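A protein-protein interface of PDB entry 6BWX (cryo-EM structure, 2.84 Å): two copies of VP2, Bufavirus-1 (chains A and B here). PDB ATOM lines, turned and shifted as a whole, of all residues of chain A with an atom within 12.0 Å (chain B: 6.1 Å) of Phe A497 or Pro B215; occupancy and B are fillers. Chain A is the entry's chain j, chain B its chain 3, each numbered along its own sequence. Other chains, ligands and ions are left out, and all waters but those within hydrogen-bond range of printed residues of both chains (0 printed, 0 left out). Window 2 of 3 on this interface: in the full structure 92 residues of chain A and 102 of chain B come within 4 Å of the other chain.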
ATOM      1  N   TRP A 249     -20.090 -24.877 -24.699  1.00  0.00           N
ATOM      2  CA  TRP A 249     -21.026 -24.346 -25.676  1.00  0.00           C
ATOM      3  C   TRP A 249     -21.023 -25.092 -26.999  1.00  0.00           C
ATOM      4  O   TRP A 249     -21.904 -24.846 -27.824  1.00  0.00           O
ATOM      5  CB  TRP A 249     -20.713 -22.876 -25.935  1.00  0.00           C
ATOM      6  CG  TRP A 249     -19.285 -22.646 -26.274  1.00  0.00           C
ATOM      7  CD1 TRP A 249     -18.280 -22.373 -25.407  1.00  0.00           C
ATOM      8  CD2 TRP A 249     -18.691 -22.698 -27.571  1.00  0.00           C
ATOM      9  NE1 TRP A 249     -17.099 -22.238 -26.079  1.00  0.00           N
ATOM     10  CE2 TRP A 249     -17.327 -22.433 -27.412  1.00  0.00           C
ATOM     11  CE3 TRP A 249     -19.181 -22.945 -28.849  1.00  0.00           C
ATOM     12  CZ2 TRP A 249     -16.452 -22.401 -28.480  1.00  0.00           C
ATOM     13  CZ3 TRP A 249     -18.317 -22.902 -29.905  1.00  0.00           C
ATOM     14  CH2 TRP A 249     -16.967 -22.638 -29.717  1.00  0.00           C
ATOM     15  N   LEU A 493      -6.582 -20.102 -15.819  1.00  0.00           N
ATOM     16  CA  LEU A 493      -5.837 -19.062 -16.502  1.00  0.00           C
ATOM     17  C   LEU A 493      -6.527 -18.723 -17.812  1.00  0.00           C
ATOM     18  O   LEU A 493      -7.258 -19.551 -18.360  1.00  0.00           O
ATOM     19  CB  LEU A 493      -4.401 -19.516 -16.765  1.00  0.00           C
ATOM     20  CG  LEU A 493      -3.594 -19.734 -15.492  1.00  0.00           C
ATOM     21  CD1 LEU A 493      -2.253 -20.335 -15.813  1.00  0.00           C
ATOM     22  CD2 LEU A 493      -3.422 -18.422 -14.773  1.00  0.00           C
ATOM     23  N   PRO A 494      -6.336 -17.511 -18.326  1.00  0.00           N
ATOM     24  CA  PRO A 494      -7.053 -17.108 -19.538  1.00  0.00           C
ATOM     25  C   PRO A 494      -6.650 -17.949 -20.738  1.00  0.00           C
ATOM     26  O   PRO A 494      -5.466 -18.099 -21.040  1.00  0.00           O
ATOM     27  CB  PRO A 494      -6.636 -15.647 -19.719  1.00  0.00           C
ATOM     28  CG  PRO A 494      -6.227 -15.212 -18.378  1.00  0.00           C
ATOM     29  CD  PRO A 494      -5.571 -16.391 -17.761  1.00  0.00           C
ATOM     30  N   ARG A 495      -7.643 -18.514 -21.416  1.00  0.00           N
ATOM     31  CA  ARG A 495      -7.424 -19.212 -22.671  1.00  0.00           C
ATOM     32  C   ARG A 495      -7.807 -18.394 -23.895  1.00  0.00           C
ATOM     33  O   ARG A 495      -7.751 -18.918 -25.008  1.00  0.00           O
ATOM     34  CB  ARG A 495      -8.165 -20.552 -22.672  1.00  0.00           C
ATOM     35  CG  ARG A 495      -7.576 -21.514 -21.663  1.00  0.00           C
ATOM     36  CD  ARG A 495      -8.234 -22.874 -21.650  1.00  0.00           C
ATOM     37  NE  ARG A 495      -7.692 -23.752 -20.620  1.00  0.00           N
ATOM     38  CZ  ARG A 495      -8.177 -24.951 -20.331  1.00  0.00           C
ATOM     39  NH1 ARG A 495      -7.626 -25.684 -19.379  1.00  0.00           N
ATOM     40  NH2 ARG A 495      -9.228 -25.409 -20.988  1.00  0.00           N
ATOM     41  N   GLN A 496      -8.215 -17.143 -23.725  1.00  0.00           N
ATOM     42  CA  GLN A 496      -8.715 -16.335 -24.823  1.00  0.00           C
ATOM     43  C   GLN A 496      -8.068 -14.959 -24.793  1.00  0.00           C
ATOM     44  O   GLN A 496      -7.416 -14.576 -23.822  1.00  0.00           O
ATOM     45  CB  GLN A 496     -10.234 -16.200 -24.750  1.00  0.00           C
ATOM     46  CG  GLN A 496     -10.672 -15.426 -23.545  1.00  0.00           C
ATOM     47  CD  GLN A 496     -12.161 -15.303 -23.433  1.00  0.00           C
ATOM     48  OE1 GLN A 496     -12.899 -16.118 -23.952  1.00  0.00           O
ATOM     49  NE2 GLN A 496     -12.613 -14.258 -22.772  1.00  0.00           N
ATOM     50  N   PHE A 497      -8.227 -14.227 -25.893  1.00  0.00           N
ATOM     51  CA  PHE A 497      -7.757 -12.848 -25.977  1.00  0.00           C
ATOM     52  C   PHE A 497      -8.740 -11.882 -25.333  1.00  0.00           C
ATOM     53  O   PHE A 497      -8.352 -11.023 -24.540  1.00  0.00           O
ATOM     54  CB  PHE A 497      -7.542 -12.482 -27.441  1.00  0.00           C
ATOM     55  CG  PHE A 497      -6.987 -11.111 -27.667  1.00  0.00           C
ATOM     56  CD1 PHE A 497      -5.630 -10.892 -27.652  1.00  0.00           C
ATOM     57  CD2 PHE A 497      -7.821 -10.047 -27.923  1.00  0.00           C
ATOM     58  CE1 PHE A 497      -5.125  -9.646 -27.884  1.00  0.00           C
ATOM     59  CE2 PHE A 497      -7.314  -8.802 -28.145  1.00  0.00           C
ATOM     60  CZ  PHE A 497      -5.966  -8.602 -28.123  1.00  0.00           C
ATOM     61  N   ASN A 498     -10.016 -12.010 -25.672  1.00  0.00           N
ATOM     62  CA  ASN A 498     -11.062 -11.100 -25.240  1.00  0.00           C
ATOM     63  C   ASN A 498     -11.425 -11.318 -23.777  1.00  0.00           C
ATOM     64  O   ASN A 498     -11.084 -12.328 -23.164  1.00  0.00           O
ATOM     65  CB  ASN A 498     -12.298 -11.264 -26.111  1.00  0.00           C
ATOM     66  CG  ASN A 498     -12.801 -12.673 -26.126  1.00  0.00           C
ATOM     67  OD1 ASN A 498     -12.062 -13.598 -25.823  1.00  0.00           O
ATOM     68  ND2 ASN A 498     -14.068 -12.849 -26.444  1.00  0.00           N
ATOM     69  N   LEU A 499     -12.115 -10.330 -23.212  1.00  0.00           N
ATOM     70  CA  LEU A 499     -12.532 -10.400 -21.818  1.00  0.00           C
ATOM     71  C   LEU A 499     -13.489 -11.555 -21.581  1.00  0.00           C
ATOM     72  O   LEU A 499     -14.440 -11.754 -22.338  1.00  0.00           O
ATOM     73  CB  LEU A 499     -13.209  -9.101 -21.406  1.00  0.00           C
ATOM     74  CG  LEU A 499     -12.371  -7.842 -21.337  1.00  0.00           C
ATOM     75  CD1 LEU A 499     -13.265  -6.675 -21.056  1.00  0.00           C
ATOM     76  CD2 LEU A 499     -11.358  -7.988 -20.249  1.00  0.00           C
ATOM     77  N   TYR A 500     -13.244 -12.308 -20.516  1.00  0.00           N
ATOM     78  CA  TYR A 500     -14.252 -13.228 -20.025  1.00  0.00           C
ATOM     79  C   TYR A 500     -15.386 -12.464 -19.364  1.00  0.00           C
ATOM     80  O   TYR A 500     -15.251 -11.303 -18.978  1.00  0.00           O
ATOM     81  CB  TYR A 500     -13.677 -14.210 -19.013  1.00  0.00           C
ATOM     82  CG  TYR A 500     -12.798 -15.277 -19.578  1.00  0.00           C
ATOM     83  CD1 TYR A 500     -13.339 -16.441 -20.078  1.00  0.00           C
ATOM     84  CD2 TYR A 500     -11.428 -15.143 -19.574  1.00  0.00           C
ATOM     85  CE1 TYR A 500     -12.546 -17.430 -20.582  1.00  0.00           C
ATOM     86  CE2 TYR A 500     -10.622 -16.129 -20.077  1.00  0.00           C
ATOM     87  CZ  TYR A 500     -11.188 -17.271 -20.579  1.00  0.00           C
ATOM     88  OH  TYR A 500     -10.388 -18.263 -21.084  1.00  0.00           O
ATOM     89  N   ASN A 501     -16.514 -13.137 -19.238  1.00  0.00           N
ATOM     90  CA  ASN A 501     -17.654 -12.624 -18.497  1.00  0.00           C
ATOM     91  C   ASN A 501     -17.689 -13.387 -17.181  1.00  0.00           C
ATOM     92  O   ASN A 501     -18.057 -14.565 -17.150  1.00  0.00           O
ATOM     93  CB  ASN A 501     -18.930 -12.805 -19.309  1.00  0.00           C
ATOM     94  CG  ASN A 501     -20.082 -12.030 -18.752  1.00  0.00           C
ATOM     95  OD1 ASN A 501     -20.097 -11.674 -17.577  1.00  0.00           O
ATOM     96  ND2 ASN A 501     -21.057 -11.742 -19.599  1.00  0.00           N
ATOM     97  N   LEU A 502     -17.325 -12.715 -16.101  1.00  0.00           N
ATOM     98  CA  LEU A 502     -16.952 -13.371 -14.860  1.00  0.00           C
ATOM     99  C   LEU A 502     -18.160 -13.676 -13.988  1.00  0.00           C
ATOM    100  O   LEU A 502     -19.235 -13.107 -14.177  1.00  0.00           O
ATOM    101  CB  LEU A 502     -15.947 -12.506 -14.113  1.00  0.00           C
ATOM    102  CG  LEU A 502     -14.511 -12.978 -14.285  1.00  0.00           C
ATOM    103  CD1 LEU A 502     -14.185 -13.098 -15.719  1.00  0.00           C
ATOM    104  CD2 LEU A 502     -13.589 -11.975 -13.671  1.00  0.00           C
ATOM    105  N   PRO A 533     -17.245 -20.252 -20.336  1.00  0.00           N
ATOM    106  CA  PRO A 533     -17.121 -21.075 -21.532  1.00  0.00           C
ATOM    107  C   PRO A 533     -15.768 -21.751 -21.588  1.00  0.00           C
ATOM    108  O   PRO A 533     -14.774 -21.251 -21.064  1.00  0.00           O
ATOM    109  CB  PRO A 533     -17.285 -20.066 -22.668  1.00  0.00           C
ATOM    110  CG  PRO A 533     -16.824 -18.804 -22.086  1.00  0.00           C
ATOM    111  CD  PRO A 533     -17.278 -18.821 -20.669  1.00  0.00           C
ATOM    112  N   ASN A 534     -15.744 -22.915 -22.224  1.00  0.00           N
ATOM    113  CA  ASN A 534     -14.494 -23.598 -22.480  1.00  0.00           C
ATOM    114  C   ASN A 534     -14.674 -24.476 -23.706  1.00  0.00           C
ATOM    115  O   ASN A 534     -15.784 -24.906 -24.022  1.00  0.00           O
ATOM    116  CB  ASN A 534     -14.055 -24.421 -21.272  1.00  0.00           C
ATOM    117  CG  ASN A 534     -12.615 -24.827 -21.349  1.00  0.00           C
ATOM    118  OD1 ASN A 534     -11.801 -24.132 -21.943  1.00  0.00           O
ATOM    119  ND2 ASN A 534     -12.285 -25.951 -20.738  1.00  0.00           N
ATOM    120  N   TYR A 535     -13.600 -24.700 -24.443  1.00  0.00           N
ATOM    121  CA  TYR A 535     -13.701 -25.520 -25.630  1.00  0.00           C
ATOM    122  C   TYR A 535     -13.867 -26.964 -25.221  1.00  0.00           C
ATOM    123  O   TYR A 535     -13.056 -27.488 -24.472  1.00  0.00           O
ATOM    124  CB  TYR A 535     -12.450 -25.381 -26.485  1.00  0.00           C
ATOM    125  CG  TYR A 535     -12.186 -23.990 -26.992  1.00  0.00           C
ATOM    126  CD1 TYR A 535     -12.973 -23.433 -27.978  1.00  0.00           C
ATOM    127  CD2 TYR A 535     -11.136 -23.244 -26.497  1.00  0.00           C
ATOM    128  CE1 TYR A 535     -12.729 -22.162 -28.448  1.00  0.00           C
ATOM    129  CE2 TYR A 535     -10.883 -21.977 -26.962  1.00  0.00           C
ATOM    130  CZ  TYR A 535     -11.684 -21.443 -27.937  1.00  0.00           C
ATOM    131  OH  TYR A 535     -11.435 -20.181 -28.402  1.00  0.00           O
ATOM    132  N   TYR B  43      -7.016 -11.492 -38.092  1.00  0.00           N
ATOM    133  CA  TYR B  43      -8.046 -12.437 -37.694  1.00  0.00           C
ATOM    134  C   TYR B  43      -9.418 -11.898 -38.050  1.00  0.00           C
ATOM    135  O   TYR B  43      -9.705 -10.719 -37.851  1.00  0.00           O
ATOM    136  CB  TYR B  43      -7.968 -12.682 -36.196  1.00  0.00           C
ATOM    137  CG  TYR B  43      -6.733 -13.402 -35.749  1.00  0.00           C
ATOM    138  CD1 TYR B  43      -5.541 -12.735 -35.601  1.00  0.00           C
ATOM    139  CD2 TYR B  43      -6.751 -14.755 -35.512  1.00  0.00           C
ATOM    140  CE1 TYR B  43      -4.413 -13.385 -35.204  1.00  0.00           C
ATOM    141  CE2 TYR B  43      -5.629 -15.406 -35.099  1.00  0.00           C
ATOM    142  CZ  TYR B  43      -4.460 -14.719 -34.958  1.00  0.00           C
ATOM    143  OH  TYR B  43      -3.324 -15.365 -34.557  1.00  0.00           O
ATOM    144  N   THR B  76      -7.948 -17.590 -38.822  1.00  0.00           N
ATOM    145  CA  THR B  76      -6.653 -17.026 -38.549  1.00  0.00           C
ATOM    146  C   THR B  76      -5.873 -16.933 -39.847  1.00  0.00           C
ATOM    147  O   THR B  76      -6.209 -17.599 -40.825  1.00  0.00           O
ATOM    148  CB  THR B  76      -5.920 -17.900 -37.549  1.00  0.00           C
ATOM    149  OG1 THR B  76      -4.732 -17.241 -37.123  1.00  0.00           O
ATOM    150  CG2 THR B  76      -5.520 -19.152 -38.201  1.00  0.00           C
ATOM    151  N   LEU B 153      -5.144 -24.432 -28.256  1.00  0.00           N
ATOM    152  CA  LEU B 153      -5.936 -23.975 -29.382  1.00  0.00           C
ATOM    153  C   LEU B 153      -7.062 -24.950 -29.674  1.00  0.00           C
ATOM    154  O   LEU B 153      -6.958 -26.140 -29.375  1.00  0.00           O
ATOM    155  CB  LEU B 153      -5.054 -23.836 -30.613  1.00  0.00           C
ATOM    156  CG  LEU B 153      -3.963 -22.776 -30.579  1.00  0.00           C
ATOM    157  CD1 LEU B 153      -3.078 -22.931 -31.784  1.00  0.00           C
ATOM    158  CD2 LEU B 153      -4.588 -21.407 -30.564  1.00  0.00           C
ATOM    159  N   TYR B 180     -11.497 -22.011 -36.904  1.00  0.00           N
ATOM    160  CA  TYR B 180     -12.288 -22.783 -35.964  1.00  0.00           C
ATOM    161  C   TYR B 180     -13.598 -22.068 -35.695  1.00  0.00           C
ATOM    162  O   TYR B 180     -13.756 -20.886 -35.998  1.00  0.00           O
ATOM    163  CB  TYR B 180     -11.522 -23.048 -34.669  1.00  0.00           C
ATOM    164  CG  TYR B 180     -11.065 -21.825 -33.922  1.00  0.00           C
ATOM    165  CD1 TYR B 180     -11.852 -21.246 -32.949  1.00  0.00           C
ATOM    166  CD2 TYR B 180      -9.830 -21.265 -34.174  1.00  0.00           C
ATOM    167  CE1 TYR B 180     -11.425 -20.145 -32.255  1.00  0.00           C
ATOM    168  CE2 TYR B 180      -9.401 -20.160 -33.492  1.00  0.00           C
ATOM    169  CZ  TYR B 180     -10.200 -19.606 -32.534  1.00  0.00           C
ATOM    170  OH  TYR B 180      -9.771 -18.498 -31.853  1.00  0.00           O
ATOM    171  N   PHE B 213     -12.283 -15.966 -28.359  1.00  0.00           N
ATOM    172  CA  PHE B 213     -11.415 -15.726 -29.498  1.00  0.00           C
ATOM    173  C   PHE B 213      -9.974 -15.852 -29.039  1.00  0.00           C
ATOM    174  O   PHE B 213      -9.492 -15.018 -28.271  1.00  0.00           O
ATOM    175  CB  PHE B 213     -11.697 -14.347 -30.078  1.00  0.00           C
ATOM    176  CG  PHE B 213     -10.581 -13.793 -30.883  1.00  0.00           C
ATOM    177  CD1 PHE B 213     -10.286 -14.290 -32.130  1.00  0.00           C
ATOM    178  CD2 PHE B 213      -9.844 -12.733 -30.403  1.00  0.00           C
ATOM    179  CE1 PHE B 213      -9.260 -13.764 -32.860  1.00  0.00           C
ATOM    180  CE2 PHE B 213      -8.825 -12.204 -31.135  1.00  0.00           C
ATOM    181  CZ  PHE B 213      -8.532 -12.718 -32.364  1.00  0.00           C
ATOM    182  N   THR B 214      -9.292 -16.883 -29.506  1.00  0.00           N
ATOM    183  CA  THR B 214      -7.908 -17.133 -29.112  1.00  0.00           C
ATOM    184  C   THR B 214      -6.973 -17.025 -30.307  1.00  0.00           C
ATOM    185  O   THR B 214      -7.037 -17.864 -31.225  1.00  0.00           O
ATOM    186  CB  THR B 214      -7.792 -18.494 -28.423  1.00  0.00           C
ATOM    187  OG1 THR B 214      -6.424 -18.772 -28.111  1.00  0.00           O
ATOM    188  CG2 THR B 214      -8.379 -19.604 -29.249  1.00  0.00           C
ATOM    189  N   PRO B 215      -6.133 -16.003 -30.372  1.00  0.00           N
ATOM    190  CA  PRO B 215      -5.144 -15.914 -31.442  1.00  0.00           C
ATOM    191  C   PRO B 215      -3.997 -16.880 -31.220  1.00  0.00           C
ATOM    192  O   PRO B 215      -3.787 -17.407 -30.130  1.00  0.00           O
ATOM    193  CB  PRO B 215      -4.653 -14.469 -31.341  1.00  0.00           C
ATOM    194  CG  PRO B 215      -5.722 -13.763 -30.657  1.00  0.00           C
ATOM    195  CD  PRO B 215      -6.237 -14.732 -29.656  1.00  0.00           C
ATOM    196  N   ILE B 216      -3.239 -17.095 -32.289  1.00  0.00           N
ATOM    197  CA  ILE B 216      -2.079 -17.966 -32.192  1.00  0.00           C
ATOM    198  C   ILE B 216      -0.971 -17.280 -31.414  1.00  0.00           C
ATOM    199  O   ILE B 216      -0.205 -17.926 -30.695  1.00  0.00           O
ATOM    200  CB  ILE B 216      -1.605 -18.369 -33.595  1.00  0.00           C
ATOM    201  CG1 ILE B 216      -2.777 -18.882 -34.420  1.00  0.00           C
ATOM    202  CG2 ILE B 216      -0.539 -19.417 -33.498  1.00  0.00           C
ATOM    203  CD1 ILE B 216      -3.474 -20.034 -33.820  1.00  0.00           C
ATOM    204  N   GLU B 217      -0.877 -15.957 -31.536  1.00  0.00           N
ATOM    205  CA  GLU B 217       0.267 -15.233 -30.998  1.00  0.00           C
ATOM    206  C   GLU B 217       0.277 -15.242 -29.479  1.00  0.00           C
ATOM    207  O   GLU B 217       1.316 -15.480 -28.859  1.00  0.00           O
ATOM    208  CB  GLU B 217       0.267 -13.805 -31.528  1.00  0.00           C
ATOM    209  CG  GLU B 217       0.641 -13.700 -32.984  1.00  0.00           C
ATOM    210  CD  GLU B 217      -0.486 -14.055 -33.917  1.00  0.00           C
ATOM    211  OE1 GLU B 217      -1.555 -14.473 -33.439  1.00  0.00           O
ATOM    212  OE2 GLU B 217      -0.303 -13.913 -35.140  1.00  0.00           O
ATOM    213  N   THR B 218      -0.867 -14.975 -28.860  1.00  0.00           N
ATOM    214  CA  THR B 218      -0.912 -14.947 -27.407  1.00  0.00           C
ATOM    215  C   THR B 218      -0.975 -16.338 -26.807  1.00  0.00           C
ATOM    216  O   THR B 218      -0.721 -16.496 -25.612  1.00  0.00           O
ATOM    217  CB  THR B 218      -2.112 -14.139 -26.931  1.00  0.00           C
ATOM    218  OG1 THR B 218      -3.314 -14.776 -27.371  1.00  0.00           O
ATOM    219  CG2 THR B 218      -2.059 -12.744 -27.508  1.00  0.00           C
ATOM    220  N   THR B 219      -1.331 -17.343 -27.597  1.00  0.00           N
ATOM    221  CA  THR B 219      -1.510 -18.682 -27.059  1.00  0.00           C
ATOM    222  C   THR B 219      -0.187 -19.413 -26.890  1.00  0.00           C
ATOM    223  O   THR B 219       0.063 -20.018 -25.844  1.00  0.00           O
ATOM    224  CB  THR B 219      -2.437 -19.476 -27.966  1.00  0.00           C
ATOM    225  OG1 THR B 219      -3.707 -18.821 -28.029  1.00  0.00           O
ATOM    226  CG2 THR B 219      -2.627 -20.864 -27.425  1.00  0.00           C
ATOM    227  N   THR B 220       0.670 -19.379 -27.904  1.00  0.00           N
ATOM    228  CA  THR B 220       1.846 -20.232 -27.937  1.00  0.00           C
ATOM    229  C   THR B 220       3.057 -19.430 -28.379  1.00  0.00           C
ATOM    230  O   THR B 220       2.941 -18.318 -28.894  1.00  0.00           O
ATOM    231  CB  THR B 220       1.632 -21.431 -28.866  1.00  0.00           C
ATOM    232  OG1 THR B 220       2.775 -22.291 -28.812  1.00  0.00           O
ATOM    233  CG2 THR B 220       1.416 -20.975 -30.283  1.00  0.00           C
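O of Asn A498 is in hydrogen-bond range of NE2 of Gln A496, 2.5 Å away. OH of Tyr B180 sits at hydrogen-bond distance from O of Thr B214 (2.9 Å). The side-chain hydroxyl (OG1) of Thr B214 is in hydrogen-bond range of the side-chain hydroxyl (OG1) of Thr B219. The side-chain amide nitrogen of Gln A496 sits close to the backbone NH of Tyr A500. NH2 of Arg A495 sits at hydrogen-bond distance from OD1 of Asn A534 (3.0 Å). The backbone carbonyl oxygen of Pro B215 sits at hydrogen-bond distance from the side-chain hydroxyl of Thr B219, 2.5 Å away.
Among the printed residues, pairs that only touch across the chains: Tyr A535 with Thr B214 (3.2 Å), Phe A497 with Pro B215 (3.4 Å), Gln A496 with Phe B213 (3.8 Å) and Tyr A535 with Tyr B180 (3.9 Å).
No position is printed for both chains. Of the 7 pairs that touch across the chains among the printed residues, none has its exchanged pair printed and touching as well.
N of Phe A497 sits at hydrogen-bond distance from O of Phe B213, at 2.8 Å. O of Arg A495 sits at hydrogen-bond distance from OG1 of Thr B214 (3.4 Å). N of Phe B213 is in hydrogen-bond range of OD1 of Asn A498, at 3.5 Å.
Of the 12 printed residues of chain B, 4 touch a printed residue of chain A. Printed residues of chain B that touch a printed residue of chain A: Tyr B180, Phe B213, Thr B214 and Pro B215. Printed residues of chain A that touch a printed residue of chain B: Arg A495, Gln A496, Phe A497, Asn A498 and Tyr A535. Hydrophobic or aromatic side chains of chain A that line the printed part of chain B: Phe A497 and Tyr A535.
Of chain B, only Phe B213 and Pro B215 come within 4 Å of Phe A497. Of chain A, only Arg A495 and Tyr A535 come within 4 Å of Thr B214. No residue of chain A comes within 4 Å of Ile B216. No residue of chain A comes within 4 Å of Glu B217. No residue of chain A comes within 4 Å of Thr B218. No residue of chain A comes within 4 Å of Thr B219. Of the printed residues of chain B, Gln A496 touches Phe B213. Printed residues of chain A within 4 Å of Tyr B180: Tyr A535. Printed residues of chain B within 4 Å of Arg A495: Thr B214. Thr B76 touches none of the printed residues of chain A. The nearest residue of chain B that does not touch Phe A497 is Thr B218 (4.03 Å). The nearest printed residue of chain B that does not touch Asn A498 is Thr B214 (5.7 Å).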
